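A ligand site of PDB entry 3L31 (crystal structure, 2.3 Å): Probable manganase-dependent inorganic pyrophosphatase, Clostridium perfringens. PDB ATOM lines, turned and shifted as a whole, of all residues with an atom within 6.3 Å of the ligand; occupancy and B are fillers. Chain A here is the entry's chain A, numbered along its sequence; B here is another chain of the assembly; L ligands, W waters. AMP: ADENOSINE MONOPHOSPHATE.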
ATOM      1  N   LYS A  36       0.472   8.241  32.822  1.00  0.00           N
ATOM      2  CA  LYS A  36       0.435   7.660  31.470  1.00  0.00           C
ATOM      3  C   LYS A  36      -0.672   6.661  31.322  1.00  0.00           C
ATOM      4  O   LYS A  36      -1.027   6.319  30.209  1.00  0.00           O
ATOM      5  CB  LYS A  36       1.727   6.951  31.112  1.00  0.00           C
ATOM      6  CG  LYS A  36       2.933   7.843  31.180  1.00  0.00           C
ATOM      7  CD  LYS A  36       4.253   7.059  31.236  1.00  0.00           C
ATOM      8  CE  LYS A  36       5.348   8.024  31.722  1.00  0.00           C
ATOM      9  NZ  LYS A  36       6.724   7.689  31.301  1.00  0.00           N
ATOM     10  N   SER A  37      -1.174   6.155  32.423  1.00  0.00           N
ATOM     11  CA  SER A  37      -2.315   5.199  32.384  1.00  0.00           C
ATOM     12  C   SER A  37      -2.976   5.241  33.748  1.00  0.00           C
ATOM     13  O   SER A  37      -2.368   5.678  34.671  1.00  0.00           O
ATOM     14  CB  SER A  37      -1.890   3.792  32.025  1.00  0.00           C
ATOM     15  OG  SER A  37      -1.071   3.206  33.047  1.00  0.00           O
ATOM     16  N   MET A  50      -7.774  -1.037  32.302  1.00  0.00           N
ATOM     17  CA  MET A  50      -6.761   0.001  32.280  1.00  0.00           C
ATOM     18  C   MET A  50      -6.997   0.919  31.127  1.00  0.00           C
ATOM     19  O   MET A  50      -7.391   0.484  30.021  1.00  0.00           O
ATOM     20  CB  MET A  50      -5.346  -0.531  32.196  1.00  0.00           C
ATOM     21  CG  MET A  50      -4.880  -1.237  33.490  1.00  0.00           C
ATOM     22  SD  MET A  50      -4.624  -0.158  34.928  1.00  0.00           S
ATOM     23  CE  MET A  50      -3.214   0.785  34.250  1.00  0.00           C
ATOM     24  N   LEU A  51      -6.775   2.218  31.416  1.00  0.00           N
ATOM     25  CA  LEU A  51      -6.904   3.257  30.426  1.00  0.00           C
ATOM     26  C   LEU A  51      -5.582   3.960  30.221  1.00  0.00           C
ATOM     27  O   LEU A  51      -5.093   4.654  31.142  1.00  0.00           O
ATOM     28  CB  LEU A  51      -7.942   4.286  30.844  1.00  0.00           C
ATOM     29  CG  LEU A  51      -8.103   5.377  29.777  1.00  0.00           C
ATOM     30  CD1 LEU A  51      -8.882   4.857  28.571  1.00  0.00           C
ATOM     31  CD2 LEU A  51      -8.757   6.606  30.300  1.00  0.00           C
ATOM     32  N   SER A  52      -5.034   3.805  29.024  1.00  0.00           N
ATOM     33  CA  SER A  52      -3.795   4.474  28.627  1.00  0.00           C
ATOM     34  C   SER A  52      -4.017   5.606  27.718  1.00  0.00           C
ATOM     35  O   SER A  52      -4.910   5.557  26.887  1.00  0.00           O
ATOM     36  CB  SER A  52      -2.879   3.565  27.822  1.00  0.00           C
ATOM     37  OG  SER A  52      -2.386   2.572  28.677  1.00  0.00           O
ATOM     38  N   THR A  53      -3.139   6.605  27.825  1.00  0.00           N
ATOM     39  CA  THR A  53      -3.122   7.723  26.882  1.00  0.00           C
ATOM     40  C   THR A  53      -3.066   7.149  25.479  1.00  0.00           C
ATOM     41  O   THR A  53      -3.551   7.759  24.550  1.00  0.00           O
ATOM     42  CB  THR A  53      -1.894   8.644  27.052  1.00  0.00           C
ATOM     43  OG1 THR A  53      -0.755   7.844  26.891  1.00  0.00           O
ATOM     44  CG2 THR A  53      -1.797   9.307  28.450  1.00  0.00           C
ATOM     45  N   SER A  54      -2.466   5.969  25.286  1.00  0.00           N
ATOM     46  CA  SER A  54      -2.423   5.391  23.930  1.00  0.00           C
ATOM     47  C   SER A  54      -3.783   4.966  23.440  1.00  0.00           C
ATOM     48  O   SER A  54      -4.097   5.109  22.249  1.00  0.00           O
ATOM     49  CB  SER A  54      -1.438   4.248  23.799  1.00  0.00           C
ATOM     50  OG  SER A  54      -1.732   3.202  24.727  1.00  0.00           O
ATOM     51  N   ASN A  55      -4.591   4.460  24.347  1.00  0.00           N
ATOM     52  CA  ASN A  55      -5.989   4.186  24.042  1.00  0.00           C
ATOM     53  C   ASN A  55      -6.769   5.446  23.603  1.00  0.00           C
ATOM     54  O   ASN A  55      -7.449   5.453  22.597  1.00  0.00           O
ATOM     55  CB  ASN A  55      -6.721   3.622  25.249  1.00  0.00           C
ATOM     56  CG  ASN A  55      -6.168   2.304  25.719  1.00  0.00           C
ATOM     57  OD1 ASN A  55      -5.913   2.136  26.926  1.00  0.00           O
ATOM     58  ND2 ASN A  55      -5.978   1.332  24.782  1.00  0.00           N
ATOM     59  N   VAL A 187     -13.183   2.405  25.527  1.00  0.00           N
ATOM     60  CA  VAL A 187     -11.824   2.628  24.980  1.00  0.00           C
ATOM     61  C   VAL A 187     -10.751   1.907  25.801  1.00  0.00           C
ATOM     62  O   VAL A 187      -9.687   1.658  25.332  1.00  0.00           O
ATOM     63  CB  VAL A 187     -11.551   4.141  24.996  1.00  0.00           C
ATOM     64  CG1 VAL A 187     -10.133   4.405  24.936  1.00  0.00           C
ATOM     65  CG2 VAL A 187     -12.297   4.846  23.825  1.00  0.00           C
ATOM     66  N   MET A 188     -11.025   1.588  27.045  1.00  0.00           N
ATOM     67  CA  MET A 188     -10.039   1.017  27.932  1.00  0.00           C
ATOM     68  C   MET A 188      -9.759  -0.406  27.575  1.00  0.00           C
ATOM     69  O   MET A 188     -10.588  -1.076  26.975  1.00  0.00           O
ATOM     70  CB  MET A 188     -10.542   1.052  29.365  1.00  0.00           C
ATOM     71  CG  MET A 188     -11.728   0.156  29.637  1.00  0.00           C
ATOM     72  SD  MET A 188     -12.401   0.431  31.257  1.00  0.00           S
ATOM     73  CE  MET A 188     -13.594  -0.924  31.483  1.00  0.00           C
ATOM     74  N   THR A 189      -8.589  -0.890  27.980  1.00  0.00           N
ATOM     75  CA  THR A 189      -8.338  -2.316  27.954  1.00  0.00           C
ATOM     76  C   THR A 189      -9.057  -3.046  29.100  1.00  0.00           C
ATOM     77  O   THR A 189      -8.958  -2.652  30.244  1.00  0.00           O
ATOM     78  CB  THR A 189      -6.827  -2.673  27.950  1.00  0.00           C
ATOM     79  OG1 THR A 189      -6.209  -2.024  26.860  1.00  0.00           O
ATOM     80  CG2 THR A 189      -6.623  -4.200  27.792  1.00  0.00           C
ATOM     81  N   ASP A 191      -9.288  -6.862  28.759  1.00  0.00           N
ATOM     82  CA  ASP A 191      -8.766  -8.232  28.752  1.00  0.00           C
ATOM     83  C   ASP A 191      -7.301  -8.327  29.154  1.00  0.00           C
ATOM     84  O   ASP A 191      -6.486  -7.436  28.881  1.00  0.00           O
ATOM     85  CB  ASP A 191      -8.917  -8.864  27.356  1.00  0.00           C
ATOM     86  CG  ASP A 191     -10.346  -8.788  26.844  1.00  0.00           C
ATOM     87  OD1 ASP A 191     -11.230  -9.420  27.477  1.00  0.00           O
ATOM     88  OD2 ASP A 191     -10.589  -8.093  25.818  1.00  0.00           O
ATOM     89  N   ASN A 192      -6.989  -9.445  29.757  1.00  0.00           N
ATOM     90  CA  ASN A 192      -5.625  -9.803  30.015  1.00  0.00           C
ATOM     91  C   ASN A 192      -4.918  -8.733  30.820  1.00  0.00           C
ATOM     92  O   ASN A 192      -3.774  -8.310  30.533  1.00  0.00           O
ATOM     93  CB  ASN A 192      -4.921 -10.095  28.679  1.00  0.00           C
ATOM     94  CG  ASN A 192      -5.672 -11.177  27.864  1.00  0.00           C
ATOM     95  OD1 ASN A 192      -5.780 -12.296  28.319  1.00  0.00           O
ATOM     96  ND2 ASN A 192      -6.263 -10.797  26.738  1.00  0.00           N
ATOM     97  N   LEU A 193      -5.606  -8.335  31.873  1.00  0.00           N
ATOM     98  CA  LEU A 193      -5.126  -7.290  32.788  1.00  0.00           C
ATOM     99  C   LEU A 193      -4.053  -7.840  33.658  1.00  0.00           C
ATOM    100  O   LEU A 193      -4.246  -8.796  34.346  1.00  0.00           O
ATOM    101  CB  LEU A 193      -6.289  -6.756  33.676  1.00  0.00           C
ATOM    102  CG  LEU A 193      -7.416  -6.142  32.885  1.00  0.00           C
ATOM    103  CD1 LEU A 193      -8.564  -5.655  33.752  1.00  0.00           C
ATOM    104  CD2 LEU A 193      -6.818  -5.024  32.038  1.00  0.00           C
ATOM    105  N   VAL A 194      -2.892  -7.232  33.622  1.00  0.00           N
ATOM    106  CA  VAL A 194      -1.818  -7.673  34.527  1.00  0.00           C
ATOM    107  C   VAL A 194      -1.855  -6.779  35.797  1.00  0.00           C
ATOM    108  O   VAL A 194      -1.503  -5.610  35.792  1.00  0.00           O
ATOM    109  CB  VAL A 194      -0.431  -7.690  33.788  1.00  0.00           C
ATOM    110  CG1 VAL A 194       0.682  -8.167  34.723  1.00  0.00           C
ATOM    111  CG2 VAL A 194      -0.509  -8.595  32.541  1.00  0.00           C
ATOM    112  N   ALA A 195      -2.373  -7.355  36.862  1.00  0.00           N
ATOM    113  CA  ALA A 195      -2.499  -6.676  38.153  1.00  0.00           C
ATOM    114  C   ALA A 195      -1.502  -7.208  39.182  1.00  0.00           C
ATOM    115  O   ALA A 195      -0.906  -8.257  39.029  1.00  0.00           O
ATOM    116  CB  ALA A 195      -3.882  -6.848  38.664  1.00  0.00           C
ATOM    117  N   ARG A 213       5.327  -4.677  28.666  1.00  0.00           N
ATOM    118  CA  ARG A 213       5.893  -3.343  28.538  1.00  0.00           C
ATOM    119  C   ARG A 213       4.968  -2.225  29.016  1.00  0.00           C
ATOM    120  O   ARG A 213       5.104  -1.069  28.610  1.00  0.00           O
ATOM    121  CB  ARG A 213       6.248  -3.104  27.064  1.00  0.00           C
ATOM    122  CG  ARG A 213       7.391  -3.950  26.598  1.00  0.00           C
ATOM    123  CD  ARG A 213       8.660  -3.497  27.253  1.00  0.00           C
ATOM    124  NE  ARG A 213       9.026  -2.143  26.838  1.00  0.00           N
ATOM    125  CZ  ARG A 213       9.986  -1.864  25.953  1.00  0.00           C
ATOM    126  NH1 ARG A 213      10.653  -2.842  25.370  1.00  0.00           N
ATOM    127  NH2 ARG A 213      10.266  -0.604  25.651  1.00  0.00           N
ATOM    128  N   TYR A 214       4.020  -2.569  29.869  1.00  0.00           N
ATOM    129  CA  TYR A 214       3.008  -1.582  30.327  1.00  0.00           C
ATOM    130  C   TYR A 214       3.572  -0.501  31.260  1.00  0.00           C
ATOM    131  O   TYR A 214       4.372  -0.768  32.123  1.00  0.00           O
ATOM    132  CB  TYR A 214       1.839  -2.296  31.024  1.00  0.00           C
ATOM    133  CG  TYR A 214       1.213  -3.386  30.175  1.00  0.00           C
ATOM    134  CD1 TYR A 214       0.849  -3.138  28.848  1.00  0.00           C
ATOM    135  CD2 TYR A 214       1.018  -4.657  30.682  1.00  0.00           C
ATOM    136  CE1 TYR A 214       0.264  -4.139  28.057  1.00  0.00           C
ATOM    137  CE2 TYR A 214       0.442  -5.654  29.902  1.00  0.00           C
ATOM    138  CZ  TYR A 214       0.073  -5.392  28.592  1.00  0.00           C
ATOM    139  OH  TYR A 214      -0.496  -6.385  27.823  1.00  0.00           O
ATOM    140  N   SER A 215       3.068   0.711  31.117  1.00  0.00           N
ATOM    141  CA  SER A 215       3.553   1.817  31.954  1.00  0.00           C
ATOM    142  C   SER A 215       3.236   1.548  33.411  1.00  0.00           C
ATOM    143  O   SER A 215       4.086   1.649  34.265  1.00  0.00           O
ATOM    144  CB  SER A 215       2.955   3.171  31.513  1.00  0.00           C
ATOM    145  OG  SER A 215       3.350   3.571  30.208  1.00  0.00           O
ATOM    146  N   ASN A 216       2.006   1.125  33.679  1.00  0.00           N
ATOM    147  CA  ASN A 216       1.562   0.899  35.041  1.00  0.00           C
ATOM    148  C   ASN A 216       0.787  -0.416  35.241  1.00  0.00           C
ATOM    149  O   ASN A 216       0.136  -0.925  34.347  1.00  0.00           O
ATOM    150  CB  ASN A 216       0.650   2.075  35.480  1.00  0.00           C
ATOM    151  CG  ASN A 216       1.389   3.427  35.512  1.00  0.00           C
ATOM    152  OD1 ASN A 216       2.353   3.573  36.231  1.00  0.00           O
ATOM    153  ND2 ASN A 216       0.919   4.403  34.755  1.00  0.00           N
ATOM    154  N   TYR A 217       0.833  -0.920  36.480  1.00  0.00           N
ATOM    155  CA  TYR A 217       0.131  -2.112  36.901  1.00  0.00           C
ATOM    156  C   TYR A 217      -0.718  -1.801  38.110  1.00  0.00           C
ATOM    157  O   TYR A 217      -0.192  -1.304  39.126  1.00  0.00           O
ATOM    158  CB  TYR A 217       1.130  -3.234  37.243  1.00  0.00           C
ATOM    159  CG  TYR A 217       2.037  -3.549  36.066  1.00  0.00           C
ATOM    160  CD1 TYR A 217       1.807  -4.683  35.254  1.00  0.00           C
ATOM    161  CD2 TYR A 217       3.090  -2.742  35.758  1.00  0.00           C
ATOM    162  CE1 TYR A 217       2.636  -4.960  34.149  1.00  0.00           C
ATOM    163  CE2 TYR A 217       3.899  -3.005  34.653  1.00  0.00           C
ATOM    164  CZ  TYR A 217       3.676  -4.142  33.864  1.00  0.00           C
ATOM    165  OH  TYR A 217       4.500  -4.407  32.758  1.00  0.00           O
ATOM    166  N   PRO A 218      -2.028  -2.054  38.014  1.00  0.00           N
ATOM    167  CA  PRO A 218      -2.904  -1.827  39.153  1.00  0.00           C
ATOM    168  C   PRO A 218      -2.568  -2.733  40.283  1.00  0.00           C
ATOM    169  O   PRO A 218      -2.295  -3.908  40.082  1.00  0.00           O
ATOM    170  CB  PRO A 218      -4.313  -2.167  38.598  1.00  0.00           C
ATOM    171  CG  PRO A 218      -4.087  -2.924  37.370  1.00  0.00           C
ATOM    172  CD  PRO A 218      -2.776  -2.437  36.812  1.00  0.00           C
ATOM    173  N   ASN B  34       4.713  -0.398  18.426  1.00  0.00           N
ATOM    174  CA  ASN B  34       4.269  -0.338  19.826  1.00  0.00           C
ATOM    175  C   ASN B  34       5.120   0.589  20.731  1.00  0.00           C
ATOM    176  O   ASN B  34       5.707   0.157  21.733  1.00  0.00           O
ATOM    177  CB  ASN B  34       4.290  -1.737  20.394  1.00  0.00           C
ATOM    178  CG  ASN B  34       2.981  -2.105  21.027  1.00  0.00           C
ATOM    179  OD1 ASN B  34       1.929  -1.986  20.380  1.00  0.00           O
ATOM    180  ND2 ASN B  34       3.006  -2.494  22.295  1.00  0.00           N
ATOM    181  N   LYS B  36       5.861   4.061  22.970  1.00  0.00           N
ATOM    182  CA  LYS B  36       5.248   5.101  23.819  1.00  0.00           C
ATOM    183  C   LYS B  36       5.783   6.451  23.374  1.00  0.00           C
ATOM    184  O   LYS B  36       5.131   7.468  23.496  1.00  0.00           O
ATOM    185  CB  LYS B  36       5.527   4.852  25.318  1.00  0.00           C
ATOM    186  CG  LYS B  36       5.011   3.513  25.837  1.00  0.00           C
ATOM    187  CD  LYS B  36       4.927   3.454  27.342  1.00  0.00           C
ATOM    188  CE  LYS B  36       4.819   2.026  27.795  1.00  0.00           C
ATOM    189  NZ  LYS B  36       4.087   1.240  26.774  1.00  0.00           N
HETATM  190  P   AMP L   1       0.595   1.449  27.969  1.00  0.00           P
HETATM  191  O1P AMP L   1       1.925   0.812  28.184  1.00  0.00           O
HETATM  192  O2P AMP L   1       0.035   1.879  29.280  1.00  0.00           O
HETATM  193  O3P AMP L   1       0.602   2.520  26.896  1.00  0.00           O
HETATM  194  O5' AMP L   1      -0.485   0.313  27.484  1.00  0.00           O
HETATM  195  C5' AMP L   1      -0.430  -0.366  26.208  1.00  0.00           C
HETATM  196  C4' AMP L   1      -1.733  -1.114  25.935  1.00  0.00           C
HETATM  197  O4' AMP L   1      -1.962  -2.067  26.983  1.00  0.00           O
HETATM  198  C3' AMP L   1      -2.954  -0.205  26.036  1.00  0.00           C
HETATM  199  O3' AMP L   1      -4.037  -0.735  25.273  1.00  0.00           O
HETATM  200  C2' AMP L   1      -3.343  -0.243  27.503  1.00  0.00           C
HETATM  201  O2' AMP L   1      -4.741  -0.016  27.705  1.00  0.00           O
HETATM  202  C1' AMP L   1      -3.013  -1.676  27.884  1.00  0.00           C
HETATM  203  N9  AMP L   1      -2.522  -1.837  29.270  1.00  0.00           N
HETATM  204  C8  AMP L   1      -1.958  -0.862  29.994  1.00  0.00           C
HETATM  205  N7  AMP L   1      -1.589  -1.282  31.214  1.00  0.00           N
HETATM  206  C5  AMP L   1      -1.946  -2.574  31.284  1.00  0.00           C
HETATM  207  C6  AMP L   1      -1.839  -3.629  32.304  1.00  0.00           C
HETATM  208  N6  AMP L   1      -1.272  -3.324  33.484  1.00  0.00           N
HETATM  209  N1  AMP L   1      -2.320  -4.885  32.025  1.00  0.00           N
HETATM  210  C2  AMP L   1      -2.880  -5.126  30.818  1.00  0.00           C
HETATM  211  N3  AMP L   1      -3.010  -4.211  29.835  1.00  0.00           N
HETATM  212  C4  AMP L   1      -2.548  -2.959  29.994  1.00  0.00           C
HETATM  213  O   HOH W   1      -2.844  -5.021  27.235  1.00  0.00           O
HETATM  214  O   HOH W   2      -0.252   1.059  31.904  1.00  0.00           O
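N of Ser 215 sits at hydrogen-bond distance from O1P of the ligand, at 3.1 Å.
The side-chain amide oxygen (OD1) of Asn 55 sits at hydrogen-bond distance from an oxygen (O2') of the ligand.
The backbone NH of Val 194 sits at hydrogen-bond distance from a nitrogen (N1) of the ligand.
O1P of the ligand is in salt-bridge range of NZ of Lys 36 of chain B, at 2.6 Å.
O of Asn 216 sits at hydrogen-bond distance from N6 of the ligand, 2.9 Å away.
The backbone carbonyl oxygen (O) of Val 194 sits at hydrogen-bond distance from a nitrogen (N6) of the ligand, 3.3 Å away.
The side-chain hydroxyl (OG1) of Thr 189 lies within hydrogen-bond range of an oxygen (O2') of the ligand, 2.6 Å away.
OG of Ser 52 lies within hydrogen-bond range of O2P of the ligand, 2.6 Å away.
O3P of the ligand is in hydrogen-bond range of OG of Ser 54 (3.3 Å).
The backbone carbonyl oxygen (O) of Arg 213 sits at hydrogen-bond distance from the side-chain amino group (NZ) of Lys 36 of chain B.
N of Tyr 214 sits at hydrogen-bond distance from OH of Tyr 217 (3.5 Å).
N of Thr 189 sits at hydrogen-bond distance from O of Met 50.
The backbone NH of Ser 52 lies within hydrogen-bond range of the side-chain amide oxygen of Asn 55 (2.8 Å).
ND2 of Asn 216 sits at hydrogen-bond distance from OG of Ser 37, at 2.9 Å.
Merely in contact with the ligand: Tyr 214, Asn 192, Met 50, Leu 193, Arg 213, Pro 218, Tyr 217 and Ser 37.
Along chain A the residues within 4 Å of the ligand span positions 37 to 218.
The nearest printed residue that does not touch the ligand is Lys 36 of chain A (4.7 Å).
Water W1 bridges a nitrogen (N3) of the ligand (2.7 Å) and the side-chain hydroxyl of Tyr 214 (2.8 Å).
Water W2 lies within hydrogen-bond range of OG of Ser 37 (2.6 Å), O2P of the ligand (2.8 Å), N of Asn 216 (2.9 Å) and N of Ser 215 (3.4 Å).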
